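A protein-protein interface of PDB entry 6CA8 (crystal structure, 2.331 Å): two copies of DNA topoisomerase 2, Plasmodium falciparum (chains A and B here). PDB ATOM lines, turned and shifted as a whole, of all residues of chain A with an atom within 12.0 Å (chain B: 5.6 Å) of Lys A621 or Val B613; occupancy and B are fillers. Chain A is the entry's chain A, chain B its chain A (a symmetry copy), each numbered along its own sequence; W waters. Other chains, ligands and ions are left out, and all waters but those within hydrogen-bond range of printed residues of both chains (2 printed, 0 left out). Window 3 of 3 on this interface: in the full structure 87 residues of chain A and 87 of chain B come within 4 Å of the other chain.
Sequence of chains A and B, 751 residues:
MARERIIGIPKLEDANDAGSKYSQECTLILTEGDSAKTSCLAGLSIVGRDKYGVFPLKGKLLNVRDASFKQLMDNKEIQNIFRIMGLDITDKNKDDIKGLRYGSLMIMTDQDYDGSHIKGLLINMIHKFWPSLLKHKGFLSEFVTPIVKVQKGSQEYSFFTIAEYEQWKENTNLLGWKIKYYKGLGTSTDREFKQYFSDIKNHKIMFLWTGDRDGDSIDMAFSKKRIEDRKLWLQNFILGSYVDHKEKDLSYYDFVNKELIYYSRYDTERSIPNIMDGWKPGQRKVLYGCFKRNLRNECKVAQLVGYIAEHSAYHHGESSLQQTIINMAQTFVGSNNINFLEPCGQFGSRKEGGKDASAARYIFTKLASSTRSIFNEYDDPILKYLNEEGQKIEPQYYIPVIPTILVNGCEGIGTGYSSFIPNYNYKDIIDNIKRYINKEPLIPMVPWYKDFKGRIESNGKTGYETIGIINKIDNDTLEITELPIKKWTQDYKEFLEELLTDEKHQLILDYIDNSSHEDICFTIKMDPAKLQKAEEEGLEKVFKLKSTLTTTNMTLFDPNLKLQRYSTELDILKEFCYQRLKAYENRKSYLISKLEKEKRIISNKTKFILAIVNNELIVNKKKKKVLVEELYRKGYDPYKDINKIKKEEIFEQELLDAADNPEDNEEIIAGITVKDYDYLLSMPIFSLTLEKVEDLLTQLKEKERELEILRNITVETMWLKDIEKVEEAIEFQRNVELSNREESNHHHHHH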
ATOM      1  N   PHE A 608     -20.526  34.324  34.512  1.00  0.00           N
ATOM      2  CA  PHE A 608     -19.762  33.328  33.760  1.00  0.00           C
ATOM      3  C   PHE A 608     -18.287  33.200  34.197  1.00  0.00           C
ATOM      4  O   PHE A 608     -17.794  32.088  34.494  1.00  0.00           O
ATOM      5  CB  PHE A 608     -19.886  33.717  32.275  1.00  0.00           C
ATOM      6  CG  PHE A 608     -19.038  32.922  31.321  1.00  0.00           C
ATOM      7  CD1 PHE A 608     -19.481  31.710  30.817  1.00  0.00           C
ATOM      8  CD2 PHE A 608     -17.842  33.440  30.848  1.00  0.00           C
ATOM      9  CE1 PHE A 608     -18.714  30.998  29.909  1.00  0.00           C
ATOM     10  CE2 PHE A 608     -17.072  32.737  29.939  1.00  0.00           C
ATOM     11  CZ  PHE A 608     -17.508  31.514  29.467  1.00  0.00           C
ATOM     12  N   ILE A 612     -16.525  30.066  36.385  1.00  0.00           N
ATOM     13  CA  ILE A 612     -15.296  29.352  36.011  1.00  0.00           C
ATOM     14  C   ILE A 612     -14.168  29.475  37.039  1.00  0.00           C
ATOM     15  O   ILE A 612     -13.544  28.486  37.427  1.00  0.00           O
ATOM     16  CB  ILE A 612     -14.736  29.841  34.668  1.00  0.00           C
ATOM     17  CG1 ILE A 612     -15.772  29.696  33.556  1.00  0.00           C
ATOM     18  CG2 ILE A 612     -13.462  29.081  34.316  1.00  0.00           C
ATOM     19  CD1 ILE A 612     -15.470  30.557  32.355  1.00  0.00           C
ATOM     20  N   ASN A 615     -14.695  27.489  40.149  1.00  0.00           N
ATOM     21  CA  ASN A 615     -14.838  26.059  39.831  1.00  0.00           C
ATOM     22  C   ASN A 615     -16.267  25.519  39.835  1.00  0.00           C
ATOM     23  O   ASN A 615     -16.474  24.304  39.839  1.00  0.00           O
ATOM     24  CB  ASN A 615     -13.991  25.209  40.788  1.00  0.00           C
ATOM     25  CG  ASN A 615     -12.524  25.589  40.766  1.00  0.00           C
ATOM     26  OD1 ASN A 615     -11.830  25.369  39.773  1.00  0.00           O
ATOM     27  ND2 ASN A 615     -12.040  26.153  41.867  1.00  0.00           N
ATOM     28  N   LEU A 617     -18.289  26.365  37.182  1.00  0.00           N
ATOM     29  CA  LEU A 617     -18.461  26.023  35.775  1.00  0.00           C
ATOM     30  C   LEU A 617     -17.171  25.468  35.167  1.00  0.00           C
ATOM     31  O   LEU A 617     -16.123  26.113  35.208  1.00  0.00           O
ATOM     32  CB  LEU A 617     -18.939  27.246  34.988  1.00  0.00           C
ATOM     33  CG  LEU A 617     -19.085  27.083  33.476  1.00  0.00           C
ATOM     34  CD1 LEU A 617     -20.148  26.043  33.164  1.00  0.00           C
ATOM     35  CD2 LEU A 617     -19.438  28.413  32.839  1.00  0.00           C
ATOM     36  N   ILE A 618     -17.264  24.265  34.604  1.00  0.00           N
ATOM     37  CA  ILE A 618     -16.132  23.608  33.956  1.00  0.00           C
ATOM     38  C   ILE A 618     -16.220  23.747  32.439  1.00  0.00           C
ATOM     39  O   ILE A 618     -17.171  23.273  31.817  1.00  0.00           O
ATOM     40  CB  ILE A 618     -16.053  22.118  34.337  1.00  0.00           C
ATOM     41  CG1 ILE A 618     -16.084  21.954  35.859  1.00  0.00           C
ATOM     42  CG2 ILE A 618     -14.800  21.484  33.752  1.00  0.00           C
ATOM     43  CD1 ILE A 618     -15.797  20.543  36.334  1.00  0.00           C
ATOM     44  N   VAL A 619     -15.215  24.385  31.849  1.00  0.00           N
ATOM     45  CA  VAL A 619     -15.111  24.484  30.396  1.00  0.00           C
ATOM     46  C   VAL A 619     -14.055  23.571  29.777  1.00  0.00           C
ATOM     47  O   VAL A 619     -14.161  23.229  28.600  1.00  0.00           O
ATOM     48  CB  VAL A 619     -14.828  25.933  29.948  1.00  0.00           C
ATOM     49  CG1 VAL A 619     -15.980  26.849  30.347  1.00  0.00           C
ATOM     50  CG2 VAL A 619     -13.507  26.426  30.525  1.00  0.00           C
ATOM     51  N   ASN A 620     -13.033  23.186  30.540  1.00  0.00           N
ATOM     52  CA  ASN A 620     -11.901  22.490  29.933  1.00  0.00           C
ATOM     53  C   ASN A 620     -12.273  21.107  29.406  1.00  0.00           C
ATOM     54  O   ASN A 620     -12.742  20.239  30.146  1.00  0.00           O
ATOM     55  CB  ASN A 620     -10.751  22.342  30.940  1.00  0.00           C
ATOM     56  CG  ASN A 620     -10.170  23.675  31.377  1.00  0.00           C
ATOM     57  OD1 ASN A 620     -10.393  24.706  30.745  1.00  0.00           O
ATOM     58  ND2 ASN A 620      -9.410  23.655  32.468  1.00  0.00           N
ATOM     59  N   LYS A 621     -12.071  20.941  28.101  1.00  0.00           N
ATOM     60  CA  LYS A 621     -12.360  19.705  27.371  1.00  0.00           C
ATOM     61  C   LYS A 621     -13.834  19.324  27.371  1.00  0.00           C
ATOM     62  O   LYS A 621     -14.173  18.151  27.233  1.00  0.00           O
ATOM     63  CB  LYS A 621     -11.518  18.535  27.879  1.00  0.00           C
ATOM     64  CG  LYS A 621     -10.062  18.876  28.089  1.00  0.00           C
ATOM     65  CD  LYS A 621      -9.183  17.827  27.427  1.00  0.00           C
ATOM     66  CE  LYS A 621      -8.832  16.690  28.353  1.00  0.00           C
ATOM     67  NZ  LYS A 621      -8.076  15.647  27.612  1.00  0.00           N
ATOM     68  N   LYS A 622     -14.708  20.310  27.527  1.00  0.00           N
ATOM     69  CA  LYS A 622     -16.136  20.045  27.497  1.00  0.00           C
ATOM     70  C   LYS A 622     -16.620  20.204  26.068  1.00  0.00           C
ATOM     71  O   LYS A 622     -16.222  21.140  25.367  1.00  0.00           O
ATOM     72  CB  LYS A 622     -16.909  20.965  28.449  1.00  0.00           C
ATOM     73  CG  LYS A 622     -18.418  20.737  28.419  1.00  0.00           C
ATOM     74  CD  LYS A 622     -19.143  21.500  29.513  1.00  0.00           C
ATOM     75  CE  LYS A 622     -19.146  20.712  30.811  1.00  0.00           C
ATOM     76  NZ  LYS A 622     -18.709  21.538  31.966  1.00  0.00           N
ATOM     77  N   LYS A 623     -17.470  19.279  25.632  1.00  0.00           N
ATOM     78  CA  LYS A 623     -18.033  19.372  24.300  1.00  0.00           C
ATOM     79  C   LYS A 623     -18.842  20.654  24.269  1.00  0.00           C
ATOM     80  O   LYS A 623     -19.515  21.006  25.235  1.00  0.00           O
ATOM     81  CB  LYS A 623     -18.914  18.165  23.985  1.00  0.00           C
ATOM     82  CG  LYS A 623     -18.173  16.852  23.787  1.00  0.00           C
ATOM     83  CD  LYS A 623     -19.170  15.726  23.532  1.00  0.00           C
ATOM     84  CE  LYS A 623     -18.521  14.504  22.904  1.00  0.00           C
ATOM     85  NZ  LYS A 623     -19.538  13.642  22.240  1.00  0.00           N
ATOM     86  N   LYS A 624     -18.766  21.349  23.149  1.00  0.00           N
ATOM     87  CA  LYS A 624     -19.350  22.670  23.036  1.00  0.00           C
ATOM     88  C   LYS A 624     -20.868  22.736  23.157  1.00  0.00           C
ATOM     89  O   LYS A 624     -21.398  23.636  23.800  1.00  0.00           O
ATOM     90  CB  LYS A 624     -18.893  23.278  21.704  1.00  0.00           C
ATOM     91  CG  LYS A 624     -19.641  22.766  20.484  1.00  0.00           C
ATOM     92  CD  LYS A 624     -19.106  23.369  19.224  1.00  0.00           C
ATOM     93  CE  LYS A 624     -18.802  22.295  18.200  1.00  0.00           C
ATOM     94  NZ  LYS A 624     -18.963  22.808  16.815  1.00  0.00           N
ATOM     95  N   LYS A 625     -21.564  21.794  22.537  1.00  0.00           N
ATOM     96  CA  LYS A 625     -23.010  21.728  22.620  1.00  0.00           C
ATOM     97  C   LYS A 625     -23.444  21.396  24.059  1.00  0.00           C
ATOM     98  O   LYS A 625     -24.480  21.864  24.531  1.00  0.00           O
ATOM     99  CB  LYS A 625     -23.500  20.722  21.590  1.00  0.00           C
ATOM    100  CG  LYS A 625     -23.451  21.396  20.211  1.00  0.00           C
ATOM    101  CD  LYS A 625     -24.047  20.637  19.048  1.00  0.00           C
ATOM    102  CE  LYS A 625     -23.865  21.476  17.779  1.00  0.00           C
ATOM    103  NZ  LYS A 625     -24.465  20.882  16.556  1.00  0.00           N
ATOM    104  N   VAL A 626     -22.635  20.588  24.744  1.00  0.00           N
ATOM    105  CA  VAL A 626     -22.855  20.257  26.153  1.00  0.00           C
ATOM    106  C   VAL A 626     -22.719  21.501  27.029  1.00  0.00           C
ATOM    107  O   VAL A 626     -23.555  21.757  27.899  1.00  0.00           O
ATOM    108  CB  VAL A 626     -21.870  19.165  26.650  1.00  0.00           C
ATOM    109  CG1 VAL A 626     -22.130  18.815  28.105  1.00  0.00           C
ATOM    110  CG2 VAL A 626     -21.963  17.922  25.784  1.00  0.00           C
ATOM    111  N   LEU A 627     -21.680  22.289  26.768  1.00  0.00           N
ATOM    112  CA  LEU A 627     -21.458  23.536  27.495  1.00  0.00           C
ATOM    113  C   LEU A 627     -22.510  24.604  27.211  1.00  0.00           C
ATOM    114  O   LEU A 627     -22.919  25.318  28.120  1.00  0.00           O
ATOM    115  CB  LEU A 627     -20.070  24.094  27.172  1.00  0.00           C
ATOM    116  CG  LEU A 627     -19.728  25.458  27.779  1.00  0.00           C
ATOM    117  CD1 LEU A 627     -19.751  25.404  29.304  1.00  0.00           C
ATOM    118  CD2 LEU A 627     -18.378  25.950  27.272  1.00  0.00           C
ATOM    119  N   VAL A 628     -22.942  24.716  25.960  1.00  0.00           N
ATOM    120  CA  VAL A 628     -24.006  25.647  25.588  1.00  0.00           C
ATOM    121  C   VAL A 628     -25.335  25.240  26.221  1.00  0.00           C
ATOM    122  O   VAL A 628     -26.089  26.087  26.725  1.00  0.00           O
ATOM    123  CB  VAL A 628     -24.170  25.735  24.052  1.00  0.00           C
ATOM    124  CG1 VAL A 628     -25.456  26.458  23.687  1.00  0.00           C
ATOM    125  CG2 VAL A 628     -22.973  26.436  23.426  1.00  0.00           C
ATOM    126  N   GLU A 630     -25.569  23.557  28.986  1.00  0.00           N
ATOM    127  CA  GLU A 630     -25.404  23.863  30.401  1.00  0.00           C
ATOM    128  C   GLU A 630     -25.536  25.355  30.723  1.00  0.00           C
ATOM    129  O   GLU A 630     -26.098  25.716  31.758  1.00  0.00           O
ATOM    130  CB  GLU A 630     -24.050  23.347  30.884  1.00  0.00           C
ATOM    131  CG  GLU A 630     -23.819  23.538  32.368  1.00  0.00           C
ATOM    132  CD  GLU A 630     -22.476  23.013  32.817  1.00  0.00           C
ATOM    133  OE1 GLU A 630     -21.808  22.324  32.018  1.00  0.00           O
ATOM    134  OE2 GLU A 630     -22.088  23.286  33.969  1.00  0.00           O
ATOM    135  N   LEU A 681     -18.359  32.971  25.330  1.00  0.00           N
ATOM    136  CA  LEU A 681     -17.277  32.064  24.935  1.00  0.00           C
ATOM    137  C   LEU A 681     -16.097  32.758  24.249  1.00  0.00           C
ATOM    138  O   LEU A 681     -14.954  32.304  24.341  1.00  0.00           O
ATOM    139  CB  LEU A 681     -17.834  30.964  24.026  1.00  0.00           C
ATOM    140  CG  LEU A 681     -19.032  30.224  24.629  1.00  0.00           C
ATOM    141  CD1 LEU A 681     -19.638  29.226  23.648  1.00  0.00           C
ATOM    142  CD2 LEU A 681     -18.631  29.541  25.924  1.00  0.00           C
ATOM    143  N   ILE A 685      -8.962  34.307  27.416  1.00  0.00           N
ATOM    144  CA  ILE A 685      -8.582  33.540  28.585  1.00  0.00           C
ATOM    145  C   ILE A 685      -8.021  34.517  29.619  1.00  0.00           C
ATOM    146  O   ILE A 685      -8.093  34.290  30.834  1.00  0.00           O
ATOM    147  CB  ILE A 685      -7.564  32.433  28.193  1.00  0.00           C
ATOM    148  CG1 ILE A 685      -8.280  31.321  27.416  1.00  0.00           C
ATOM    149  CG2 ILE A 685      -6.850  31.871  29.415  1.00  0.00           C
ATOM    150  CD1 ILE A 685      -7.351  30.394  26.646  1.00  0.00           C
ATOM    151  N   LEU A 688      -9.825  35.669  32.816  1.00  0.00           N
ATOM    152  CA  LEU A 688      -9.807  34.886  34.052  1.00  0.00           C
ATOM    153  C   LEU A 688      -8.719  35.289  35.043  1.00  0.00           C
ATOM    154  O   LEU A 688      -8.762  34.879  36.197  1.00  0.00           O
ATOM    155  CB  LEU A 688      -9.682  33.392  33.733  1.00  0.00           C
ATOM    156  CG  LEU A 688     -10.652  32.794  32.714  1.00  0.00           C
ATOM    157  CD1 LEU A 688     -10.156  31.448  32.231  1.00  0.00           C
ATOM    158  CD2 LEU A 688     -12.043  32.671  33.321  1.00  0.00           C
ATOM    159  N   PHE B 608       0.361  25.896  25.410  1.00  0.00           N
ATOM    160  CA  PHE B 608      -0.386  26.730  26.353  1.00  0.00           C
ATOM    161  C   PHE B 608      -1.788  26.187  26.705  1.00  0.00           C
ATOM    162  O   PHE B 608      -2.142  26.035  27.896  1.00  0.00           O
ATOM    163  CB  PHE B 608      -0.458  28.135  25.726  1.00  0.00           C
ATOM    164  CG  PHE B 608      -1.327  29.126  26.450  1.00  0.00           C
ATOM    165  CD1 PHE B 608      -0.833  29.862  27.514  1.00  0.00           C
ATOM    166  CD2 PHE B 608      -2.610  29.395  25.996  1.00  0.00           C
ATOM    167  CE1 PHE B 608      -1.624  30.802  28.155  1.00  0.00           C
ATOM    168  CE2 PHE B 608      -3.405  30.335  26.627  1.00  0.00           C
ATOM    169  CZ  PHE B 608      -2.913  31.040  27.708  1.00  0.00           C
ATOM    170  N   ILE B 609      -2.544  25.810  25.675  1.00  0.00           N
ATOM    171  CA  ILE B 609      -3.855  25.187  25.848  1.00  0.00           C
ATOM    172  C   ILE B 609      -3.819  23.828  26.541  1.00  0.00           C
ATOM    173  O   ILE B 609      -4.633  23.560  27.432  1.00  0.00           O
ATOM    174  CB  ILE B 609      -4.574  25.021  24.493  1.00  0.00           C
ATOM    175  CG1 ILE B 609      -4.755  26.382  23.818  1.00  0.00           C
ATOM    176  CG2 ILE B 609      -5.922  24.330  24.674  1.00  0.00           C
ATOM    177  CD1 ILE B 609      -5.675  27.327  24.566  1.00  0.00           C
ATOM    178  N   LEU B 610      -2.869  22.981  26.147  1.00  0.00           N
ATOM    179  CA  LEU B 610      -2.730  21.673  26.778  1.00  0.00           C
ATOM    180  C   LEU B 610      -2.363  21.828  28.244  1.00  0.00           C
ATOM    181  O   LEU B 610      -2.891  21.117  29.096  1.00  0.00           O
ATOM    182  CB  LEU B 610      -1.691  20.819  26.050  1.00  0.00           C
ATOM    183  CG  LEU B 610      -2.164  20.256  24.707  1.00  0.00           C
ATOM    184  CD1 LEU B 610      -1.095  19.384  24.079  1.00  0.00           C
ATOM    185  CD2 LEU B 610      -3.464  19.477  24.873  1.00  0.00           C
ATOM    186  N   ALA B 611      -1.464  22.763  28.535  1.00  0.00           N
ATOM    187  CA  ALA B 611      -1.044  22.992  29.911  1.00  0.00           C
ATOM    188  C   ALA B 611      -2.191  23.465  30.802  1.00  0.00           C
ATOM    189  O   ALA B 611      -2.340  22.981  31.927  1.00  0.00           O
ATOM    190  CB  ALA B 611       0.093  23.997  29.952  1.00  0.00           C
ATOM    191  N   ILE B 612      -3.011  24.397  30.312  1.00  0.00           N
ATOM    192  CA  ILE B 612      -4.203  24.770  31.087  1.00  0.00           C
ATOM    193  C   ILE B 612      -5.220  23.638  31.247  1.00  0.00           C
ATOM    194  O   ILE B 612      -5.707  23.363  32.345  1.00  0.00           O
ATOM    195  CB  ILE B 612      -4.946  25.957  30.457  1.00  0.00           C
ATOM    196  CG1 ILE B 612      -4.027  27.168  30.316  1.00  0.00           C
ATOM    197  CG2 ILE B 612      -6.175  26.312  31.286  1.00  0.00           C
ATOM    198  CD1 ILE B 612      -4.533  28.177  29.316  1.00  0.00           C
ATOM    199  N   VAL B 613      -5.511  22.973  30.134  1.00  0.00           N
ATOM    200  CA  VAL B 613      -6.454  21.861  30.085  1.00  0.00           C
ATOM    201  C   VAL B 613      -5.998  20.636  30.889  1.00  0.00           C
ATOM    202  O   VAL B 613      -6.827  19.888  31.414  1.00  0.00           O
ATOM    203  CB  VAL B 613      -6.739  21.479  28.606  1.00  0.00           C
ATOM    204  CG1 VAL B 613      -6.610  19.984  28.364  1.00  0.00           C
ATOM    205  CG2 VAL B 613      -8.100  22.019  28.163  1.00  0.00           C
ATOM    206  N   ASN B 614      -4.686  20.455  31.024  1.00  0.00           N
ATOM    207  CA  ASN B 614      -4.158  19.340  31.810  1.00  0.00           C
ATOM    208  C   ASN B 614      -3.805  19.739  33.246  1.00  0.00           C
ATOM    209  O   ASN B 614      -3.197  18.956  33.978  1.00  0.00           O
ATOM    210  CB  ASN B 614      -2.919  18.747  31.126  1.00  0.00           C
ATOM    211  CG  ASN B 614      -3.263  17.914  29.900  1.00  0.00           C
ATOM    212  OD1 ASN B 614      -4.342  17.329  29.814  1.00  0.00           O
ATOM    213  ND2 ASN B 614      -2.344  17.863  28.941  1.00  0.00           N
ATOM    214  N   ASN B 615      -4.184  20.961  33.625  1.00  0.00           N
ATOM    215  CA  ASN B 615      -3.945  21.522  34.964  1.00  0.00           C
ATOM    216  C   ASN B 615      -2.482  21.738  35.341  1.00  0.00           C
ATOM    217  O   ASN B 615      -2.165  21.954  36.513  1.00  0.00           O
ATOM    218  CB  ASN B 615      -4.604  20.646  36.039  1.00  0.00           C
ATOM    219  CG  ASN B 615      -6.093  20.471  35.820  1.00  0.00           C
ATOM    220  OD1 ASN B 615      -6.867  21.419  35.955  1.00  0.00           O
ATOM    221  ND2 ASN B 615      -6.505  19.253  35.489  1.00  0.00           N
ATOM    222  N   LEU B 617      -0.841  24.388  33.881  1.00  0.00           N
ATOM    223  CA  LEU B 617      -0.791  25.842  33.979  1.00  0.00           C
ATOM    224  C   LEU B 617      -2.083  26.413  34.569  1.00  0.00           C
ATOM    225  O   LEU B 617      -3.175  26.171  34.054  1.00  0.00           O
ATOM    226  CB  LEU B 617      -0.514  26.456  32.604  1.00  0.00           C
ATOM    227  CG  LEU B 617      -0.517  27.981  32.514  1.00  0.00           C
ATOM    228  CD1 LEU B 617       0.597  28.556  33.372  1.00  0.00           C
ATOM    229  CD2 LEU B 617      -0.358  28.418  31.071  1.00  0.00           C
ATOM    230  N   LEU B 688     -10.539  26.363  24.974  1.00  0.00           N
ATOM    231  CA  LEU B 688     -10.352  25.277  25.938  1.00  0.00           C
ATOM    232  C   LEU B 688     -11.360  24.138  25.813  1.00  0.00           C
ATOM    233  O   LEU B 688     -11.156  23.076  26.390  1.00  0.00           O
ATOM    234  CB  LEU B 688     -10.374  25.826  27.368  1.00  0.00           C
ATOM    235  CG  LEU B 688      -9.469  27.014  27.692  1.00  0.00           C
ATOM    236  CD1 LEU B 688      -9.888  27.666  28.993  1.00  0.00           C
ATOM    237  CD2 LEU B 688      -8.015  26.565  27.758  1.00  0.00           C
ATOM    238  N   THR B 689     -12.433  24.359  25.059  1.00  0.00           N
ATOM    239  CA  THR B 689     -13.445  23.326  24.844  1.00  0.00           C
ATOM    240  C   THR B 689     -12.904  22.214  23.930  1.00  0.00           C
ATOM    241  O   THR B 689     -11.967  22.438  23.163  1.00  0.00           O
ATOM    242  CB  THR B 689     -14.733  23.923  24.258  1.00  0.00           C
ATOM    243  OG1 THR B 689     -14.448  24.537  22.995  1.00  0.00           O
ATOM    244  CG2 THR B 689     -15.295  24.991  25.197  1.00  0.00           C
ATOM    245  N   LEU B 690     -13.519  21.033  23.993  1.00  0.00           N
ATOM    246  CA  LEU B 690     -12.938  19.804  23.435  1.00  0.00           C
ATOM    247  C   LEU B 690     -12.652  19.792  21.926  1.00  0.00           C
ATOM    248  O   LEU B 690     -11.556  19.404  21.503  1.00  0.00           O
ATOM    249  CB  LEU B 690     -13.856  18.620  23.754  1.00  0.00           C
ATOM    250  CG  LEU B 690     -13.395  17.270  23.200  1.00  0.00           C
ATOM    251  CD1 LEU B 690     -12.042  16.876  23.788  1.00  0.00           C
ATOM    252  CD2 LEU B 690     -14.445  16.198  23.450  1.00  0.00           C
ATOM    253  N   VAL B 693      -9.796  22.119  21.132  1.00  0.00           N
ATOM    254  CA  VAL B 693      -8.524  21.505  21.505  1.00  0.00           C
ATOM    255  C   VAL B 693      -8.073  20.462  20.490  1.00  0.00           C
ATOM    256  O   VAL B 693      -6.897  20.415  20.098  1.00  0.00           O
ATOM    257  CB  VAL B 693      -8.625  20.841  22.899  1.00  0.00           C
ATOM    258  CG1 VAL B 693      -7.342  20.096  23.243  1.00  0.00           C
ATOM    259  CG2 VAL B 693      -8.939  21.881  23.965  1.00  0.00           C
HETATM  260  O   HOH W   1      -5.542  16.525  26.718  1.00  0.00           O
HETATM  261  O   HOH W   2      -8.982  20.705  33.524  1.00  0.00           O
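The backbone carbonyl oxygen (O) of Lys A622 is in hydrogen-bond range of the backbone NH (N) of Leu B690. N of Lys A621 lies within hydrogen-bond range of O of Leu B688.
The side-chain amino group (NZ) of Lys A622 lies within salt-bridge range of the side-chain carboxylate (OE1) of Glu A630 (3.2 Å).
Leu B688 touches Val A619 (O to O, 3.7 Å). Thr B689 touches Val A619 (CA to O, 3.8 Å). Asn A620 touches Ile B612. Val B613 touches Asn A620 (CG2 to CB, 3.9 Å). Asn A620 touches Leu B688. CD of Lys A621 touches CG1 of Val B613, at 3.5 Å. Leu B690 touches Lys A621 (CB to O, 3.5 Å). CB of Thr B689 touches O of Lys A622, 3.3 Å away. Lys A623 touches Leu B690. Thr B689 touches Leu A627 (CG2 to CD2, 3.8 Å).
Of chain B, only Val B613, Leu B688 and Leu B690 come within 4 Å of Lys A621. Of chain A, only Asn A620 (3.9 Å) and Lys A621 (3.5 Å) come within 4 Å of Val B613. No residue of chain A comes within 4 Å of Leu B610. No residue of chain A comes within 4 Å of Ala B611. Ile B612 touches one residue of chain A. No residue of chain A comes within 4 Å of Asn B614. No residue of chain A comes within 4 Å of Asn B615. Leu B688 touches just these residues of chain A: Val A619, Asn A620 and Lys A621. Thr B689 touches just these residues of chain A: Val A619 (3.8 Å), Lys A622 (3.3 Å) and Leu A627 (3.8 Å). Of chain A, only Lys A621, Lys A622 and Lys A623 come within 4 Å of Leu B690. Printed residues of chain B within 4 Å of Lys A623: Leu B690. Of the printed residues of chain B, Asn A620 touches Ile B612, Val B613 and Leu B688. Ile A618 touches none of the printed residues of chain B. The nearest residue of chain B that does not touch Lys A621 is Thr B689 (4.3 Å).
Hydrophobic or aromatic side chains of chain A within 4 Å of the printed part of chain B: Leu A627 and Ile A685. Of the 13 printed residues of chain B, 6 touch a printed residue of chain A. Among the printed residues, 13 pairs touch across the chains.
5 positions are printed for both chains. Of the 13 pairs that touch across the chains among the printed residues, none has its exchanged pair printed and touching as well.
Water W1 lies within hydrogen-bond range of NZ of Lys A621 (2.8 Å) and OD1 of Asn B614 (3.4 Å). Water W2 lies within hydrogen-bond range of O of Val B613, ND2 of Asn A620 and OD1 of Asn B615.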
